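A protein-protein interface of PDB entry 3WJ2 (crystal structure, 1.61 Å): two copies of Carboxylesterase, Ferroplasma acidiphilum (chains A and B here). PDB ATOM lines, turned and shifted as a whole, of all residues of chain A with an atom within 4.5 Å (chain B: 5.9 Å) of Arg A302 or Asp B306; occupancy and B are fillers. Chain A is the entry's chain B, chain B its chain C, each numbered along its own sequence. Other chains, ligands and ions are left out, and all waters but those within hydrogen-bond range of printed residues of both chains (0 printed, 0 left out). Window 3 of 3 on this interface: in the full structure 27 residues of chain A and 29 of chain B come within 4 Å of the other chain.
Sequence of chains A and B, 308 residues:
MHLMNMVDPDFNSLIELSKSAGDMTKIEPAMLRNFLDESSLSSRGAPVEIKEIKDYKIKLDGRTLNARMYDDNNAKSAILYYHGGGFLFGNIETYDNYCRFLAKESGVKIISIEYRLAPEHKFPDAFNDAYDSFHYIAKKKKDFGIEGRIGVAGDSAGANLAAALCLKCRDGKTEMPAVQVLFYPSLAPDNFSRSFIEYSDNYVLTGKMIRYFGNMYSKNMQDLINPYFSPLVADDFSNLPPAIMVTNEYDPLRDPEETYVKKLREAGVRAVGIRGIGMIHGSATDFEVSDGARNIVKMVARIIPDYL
Arg B302 touches its own counterpart, Arg A302.
Arg A302 touches Ile B303, and with the chains exchanged Ile A303 touches Arg B302.
4 positions are printed for both chains.
Of the 7 pairs that touch across the chains among the printed residues, 3 have their exchanged pair printed and touching as well.
Printed residues of chain B within 4 Å of Lys A298: Ile B303 (3.9 Å) and Asp B306 (2.5 Å).
Of the printed residues of chain B, Met A299 touches Ile B303.
Arg A302 touches just these residues of chain B: Arg B302, Ile B303 and Asp B306.
Of the printed residues of chain B, Ile A303 touches Arg B302.
Printed residues of chain A within 4 Å of Ile B303: Lys A298 (3.9 Å), Met A299 (3.7 Å) and Arg A302 (3.8 Å).
Ile B304 touches none of the printed residues of chain A.
Of the printed residues of chain A, Asp B306 touches Lys A298 and Arg A302.
The nearest printed residue of chain B that does not touch Lys A298 is Arg B302 (6.1 Å).
The side-chain amino group (NZ) of Lys A298 lies within salt-bridge range of the side-chain carboxylate (OD2) of Asp B306 (2.5 Å).
The backbone carbonyl oxygen (O) of Arg A302 lies within hydrogen-bond range of the guanidinium group (NH1) of Arg B302, at 2.8 Å.
NH2 of Arg A302 lies within salt-bridge range of OD2 of Asp B306, 2.8 Å away.
Lys A298 touches Ile B303.
Ile B303 touches Met A299.
Ile B303 touches Arg A302.
NH1 of Arg B302 touches CA of Ile A303, 3.8 Å away.
The side-chain carboxylate (OE1) of Glu A105 is in salt-bridge range of the guanidinium group (NH2) of Arg A302.
Printed residues of chain A that touch a printed residue of chain B: Lys A298, Met A299, Arg A302 and Ile A303.
Of the 7 printed residues of chain B, 3 touch a printed residue of chain A.
Printed residues of chain B that touch a printed residue of chain A: Arg B302, Ile B303 and Asp B306.
Hydrophobic or aromatic side chains of chain B that line the printed part of chain A: Ile B303.
Among the printed residues, Asp or Glu carboxylates within 4 Å of a Lys or Arg side-chain nitrogen of the other chain: Lys A298 with Asp B306 (2.5 Å) and Arg A302 with Asp B306 (2.8 Å).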
ATOM      1  N   GLU A 105     -24.804  27.858 -30.109  1.00  0.00           N
ATOM      2  CA  GLU A 105     -23.916  26.894 -29.497  1.00  0.00           C
ATOM      3  C   GLU A 105     -23.703  27.011 -27.975  1.00  0.00           C
ATOM      4  O   GLU A 105     -23.452  26.019 -27.280  1.00  0.00           O
ATOM      5  CB  GLU A 105     -22.548  26.982 -30.199  1.00  0.00           C
ATOM      6  CG  GLU A 105     -22.599  26.612 -31.701  1.00  0.00           C
ATOM      7  CD  GLU A 105     -23.023  25.172 -31.953  1.00  0.00           C
ATOM      8  OE1 GLU A 105     -22.864  24.321 -31.059  1.00  0.00           O
ATOM      9  OE2 GLU A 105     -23.671  24.933 -33.029  1.00  0.00           O
ATOM     10  N   LYS A 298     -17.167  26.316 -31.532  1.00  0.00           N
ATOM     11  CA  LYS A 298     -18.098  25.453 -30.789  1.00  0.00           C
ATOM     12  C   LYS A 298     -17.561  24.994 -29.414  1.00  0.00           C
ATOM     13  O   LYS A 298     -18.264  24.974 -28.398  1.00  0.00           O
ATOM     14  CB  LYS A 298     -18.385  24.172 -31.618  1.00  0.00           C
ATOM     15  CG  LYS A 298     -19.327  24.404 -32.692  1.00  0.00           C
ATOM     16  CD  LYS A 298     -19.460  23.107 -33.630  1.00  0.00           C
ATOM     17  CE  LYS A 298     -19.938  21.958 -32.954  1.00  0.00           C
ATOM     18  NZ  LYS A 298     -20.334  21.082 -34.131  1.00  0.00           N
ATOM     19  N   MET A 299     -16.234  24.656 -29.381  1.00  0.00           N
ATOM     20  CA  MET A 299     -15.537  24.196 -28.160  1.00  0.00           C
ATOM     21  C   MET A 299     -15.714  25.331 -27.103  1.00  0.00           C
ATOM     22  O   MET A 299     -16.091  25.057 -25.965  1.00  0.00           O
ATOM     23  CB  MET A 299     -14.027  23.952 -28.439  1.00  0.00           C
ATOM     24  CG  MET A 299     -13.835  22.612 -28.931  1.00  0.00           C
ATOM     25  SD  MET A 299     -11.957  22.696 -29.326  1.00  0.00           S
ATOM     26  CE  MET A 299     -12.187  21.042 -29.196  1.00  0.00           C
ATOM     27  N   VAL A 300     -15.371  26.518 -27.460  1.00  0.00           N
ATOM     28  CA  VAL A 300     -15.421  27.653 -26.528  1.00  0.00           C
ATOM     29  C   VAL A 300     -16.855  27.929 -26.124  1.00  0.00           C
ATOM     30  O   VAL A 300     -17.175  28.045 -24.935  1.00  0.00           O
ATOM     31  CB  VAL A 300     -14.753  28.869 -27.158  1.00  0.00           C
ATOM     32  CG1 VAL A 300     -14.979  30.070 -26.260  1.00  0.00           C
ATOM     33  CG2 VAL A 300     -13.210  28.589 -27.299  1.00  0.00           C
ATOM     34  N   ALA A 301     -17.737  28.028 -27.142  1.00  0.00           N
ATOM     35  CA  ALA A 301     -19.091  28.424 -26.836  1.00  0.00           C
ATOM     36  C   ALA A 301     -19.753  27.436 -25.907  1.00  0.00           C
ATOM     37  O   ALA A 301     -20.559  27.879 -25.101  1.00  0.00           O
ATOM     38  CB  ALA A 301     -19.885  28.523 -28.221  1.00  0.00           C
ATOM     39  N   ARG A 302     -19.456  26.125 -26.047  1.00  0.00           N
ATOM     40  CA  ARG A 302     -20.038  25.134 -25.224  1.00  0.00           C
ATOM     41  C   ARG A 302     -19.554  25.034 -23.805  1.00  0.00           C
ATOM     42  O   ARG A 302     -20.252  24.407 -22.992  1.00  0.00           O
ATOM     43  CB  ARG A 302     -20.068  23.756 -25.959  1.00  0.00           C
ATOM     44  CG  ARG A 302     -20.897  23.807 -27.198  1.00  0.00           C
ATOM     45  CD  ARG A 302     -20.812  22.417 -27.935  1.00  0.00           C
ATOM     46  NE  ARG A 302     -21.617  22.544 -29.173  1.00  0.00           N
ATOM     47  CZ  ARG A 302     -21.879  21.500 -29.952  1.00  0.00           C
ATOM     48  NH1 ARG A 302     -21.357  20.313 -29.647  1.00  0.00           N
ATOM     49  NH2 ARG A 302     -22.652  21.628 -31.023  1.00  0.00           N
ATOM     50  N   ILE A 303     -18.437  25.707 -23.471  1.00  0.00           N
ATOM     51  CA  ILE A 303     -17.989  25.734 -22.062  1.00  0.00           C
ATOM     52  C   ILE A 303     -18.373  27.084 -21.440  1.00  0.00           C
ATOM     53  O   ILE A 303     -18.350  27.150 -20.247  1.00  0.00           O
ATOM     54  CB  ILE A 303     -16.508  25.389 -21.829  1.00  0.00           C
ATOM     55  CG1 ILE A 303     -15.478  26.352 -22.526  1.00  0.00           C
ATOM     56  CG2 ILE A 303     -16.303  23.916 -22.359  1.00  0.00           C
ATOM     57  CD1 ILE A 303     -14.078  26.219 -21.848  1.00  0.00           C
ATOM     58  N   ILE A 304     -18.707  28.097 -22.246  1.00  0.00           N
ATOM     59  CA  ILE A 304     -19.137  29.391 -21.661  1.00  0.00           C
ATOM     60  C   ILE A 304     -20.244  29.279 -20.551  1.00  0.00           C
ATOM     61  O   ILE A 304     -20.075  29.910 -19.483  1.00  0.00           O
ATOM     62  CB  ILE A 304     -19.546  30.359 -22.731  1.00  0.00           C
ATOM     63  CG1 ILE A 304     -18.320  30.931 -23.471  1.00  0.00           C
ATOM     64  CG2 ILE A 304     -20.421  31.521 -22.138  1.00  0.00           C
ATOM     65  CD1 ILE A 304     -18.685  31.761 -24.712  1.00  0.00           C
ATOM     66  N   PRO A 305     -21.280  28.457 -20.767  1.00  0.00           N
ATOM     67  CA  PRO A 305     -22.335  28.417 -19.774  1.00  0.00           C
ATOM     68  C   PRO A 305     -21.848  27.985 -18.407  1.00  0.00           C
ATOM     69  O   PRO A 305     -22.456  28.456 -17.401  1.00  0.00           O
ATOM     70  CB  PRO A 305     -23.412  27.470 -20.406  1.00  0.00           C
ATOM     71  CG  PRO A 305     -22.769  26.804 -21.484  1.00  0.00           C
ATOM     72  CD  PRO A 305     -21.595  27.631 -21.957  1.00  0.00           C
ATOM     73  N   ARG B 302     -17.345  18.019 -25.280  1.00  0.00           N
ATOM     74  CA  ARG B 302     -18.666  18.611 -25.615  1.00  0.00           C
ATOM     75  C   ARG B 302     -18.900  18.667 -27.112  1.00  0.00           C
ATOM     76  O   ARG B 302     -20.022  18.965 -27.526  1.00  0.00           O
ATOM     77  CB  ARG B 302     -18.875  19.981 -24.897  1.00  0.00           C
ATOM     78  CG  ARG B 302     -19.129  19.705 -23.465  1.00  0.00           C
ATOM     79  CD  ARG B 302     -19.343  21.019 -22.696  1.00  0.00           C
ATOM     80  NE  ARG B 302     -19.469  20.702 -21.268  1.00  0.00           N
ATOM     81  CZ  ARG B 302     -19.826  21.609 -20.339  1.00  0.00           C
ATOM     82  NH1 ARG B 302     -20.171  22.876 -20.699  1.00  0.00           N
ATOM     83  NH2 ARG B 302     -19.870  21.226 -19.040  1.00  0.00           N
ATOM     84  N   ILE B 303     -17.822  18.552 -27.909  1.00  0.00           N
ATOM     85  CA  ILE B 303     -18.033  18.514 -29.395  1.00  0.00           C
ATOM     86  C   ILE B 303     -18.065  17.072 -29.950  1.00  0.00           C
ATOM     87  O   ILE B 303     -18.500  16.916 -31.104  1.00  0.00           O
ATOM     88  CB  ILE B 303     -17.174  19.429 -30.243  1.00  0.00           C
ATOM     89  CG1 ILE B 303     -15.692  18.988 -30.187  1.00  0.00           C
ATOM     90  CG2 ILE B 303     -17.311  20.890 -29.725  1.00  0.00           C
ATOM     91  CD1 ILE B 303     -14.865  19.564 -31.344  1.00  0.00           C
ATOM     92  N   ILE B 304     -17.663  16.109 -29.170  1.00  0.00           N
ATOM     93  CA  ILE B 304     -17.692  14.660 -29.635  1.00  0.00           C
ATOM     94  C   ILE B 304     -19.079  14.307 -30.237  1.00  0.00           C
ATOM     95  O   ILE B 304     -19.113  13.623 -31.272  1.00  0.00           O
ATOM     96  CB  ILE B 304     -17.238  13.727 -28.486  1.00  0.00           C
ATOM     97  CG1 ILE B 304     -15.720  13.813 -28.402  1.00  0.00           C
ATOM     98  CG2 ILE B 304     -17.670  12.227 -28.754  1.00  0.00           C
ATOM     99  CD1 ILE B 304     -15.142  12.978 -27.291  1.00  0.00           C
ATOM    100  N   PRO B 305     -20.193  14.657 -29.526  1.00  0.00           N
ATOM    101  CA  PRO B 305     -21.481  14.143 -30.017  1.00  0.00           C
ATOM    102  C   PRO B 305     -21.852  14.589 -31.362  1.00  0.00           C
ATOM    103  O   PRO B 305     -22.578  13.836 -32.064  1.00  0.00           O
ATOM    104  CB  PRO B 305     -22.511  14.620 -28.968  1.00  0.00           C
ATOM    105  CG  PRO B 305     -21.744  15.565 -28.056  1.00  0.00           C
ATOM    106  CD  PRO B 305     -20.339  15.269 -28.174  1.00  0.00           C
ATOM    107  N   ASP B 306     -21.348  15.715 -31.841  1.00  0.00           N
ATOM    108  CA  ASP B 306     -21.633  16.181 -33.171  1.00  0.00           C
ATOM    109  C   ASP B 306     -21.100  15.254 -34.269  1.00  0.00           C
ATOM    110  O   ASP B 306     -21.618  15.290 -35.377  1.00  0.00           O
ATOM    111  CB  ASP B 306     -21.105  17.591 -33.358  1.00  0.00           C
ATOM    112  CG  ASP B 306     -21.856  18.608 -32.477  1.00  0.00           C
ATOM    113  OD1 ASP B 306     -22.326  18.288 -31.384  1.00  0.00           O
ATOM    114  OD2 ASP B 306     -22.007  19.721 -32.913  1.00  0.00           O
ATOM    115  N   TYR B 307     -20.087  14.429 -33.990  1.00  0.00           N
ATOM    116  CA  TYR B 307     -19.510  13.497 -34.979  1.00  0.00           C
ATOM    117  C   TYR B 307     -20.293  12.155 -34.988  1.00  0.00           C
ATOM    118  O   TYR B 307     -19.950  11.311 -35.855  1.00  0.00           O
ATOM    119  CB  TYR B 307     -18.047  13.169 -34.582  1.00  0.00           C
ATOM    120  CG  TYR B 307     -17.165  14.366 -34.757  1.00  0.00           C
ATOM    121  CD1 TYR B 307     -16.394  14.540 -35.912  1.00  0.00           C
ATOM    122  CD2 TYR B 307     -17.040  15.302 -33.688  1.00  0.00           C
ATOM    123  CE1 TYR B 307     -15.535  15.642 -36.079  1.00  0.00           C
ATOM    124  CE2 TYR B 307     -16.260  16.430 -33.856  1.00  0.00           C
ATOM    125  CZ  TYR B 307     -15.441  16.560 -34.998  1.00  0.00           C
ATOM    126  OH  TYR B 307     -14.654  17.692 -35.077  1.00  0.00           O
ATOM    127  N   LEU B 308     -21.236  11.938 -34.071  1.00  0.00           N
ATOM    128  CA  LEU B 308     -21.804  10.569 -33.786  1.00  0.00           C
ATOM    129  C   LEU B 308     -23.316  10.453 -34.141  1.00  0.00           C
ATOM    130  O   LEU B 308     -23.771  11.347 -34.883  1.00  0.00           O
ATOM    131  CB  LEU B 308     -21.583  10.155 -32.353  1.00  0.00           C
ATOM    132  CG  LEU B 308     -20.073  10.110 -32.034  1.00  0.00           C
ATOM    133  CD1 LEU B 308     -20.009   9.764 -30.544  1.00  0.00           C
ATOM    134  CD2 LEU B 308     -19.304   9.079 -32.844  1.00  0.00           C
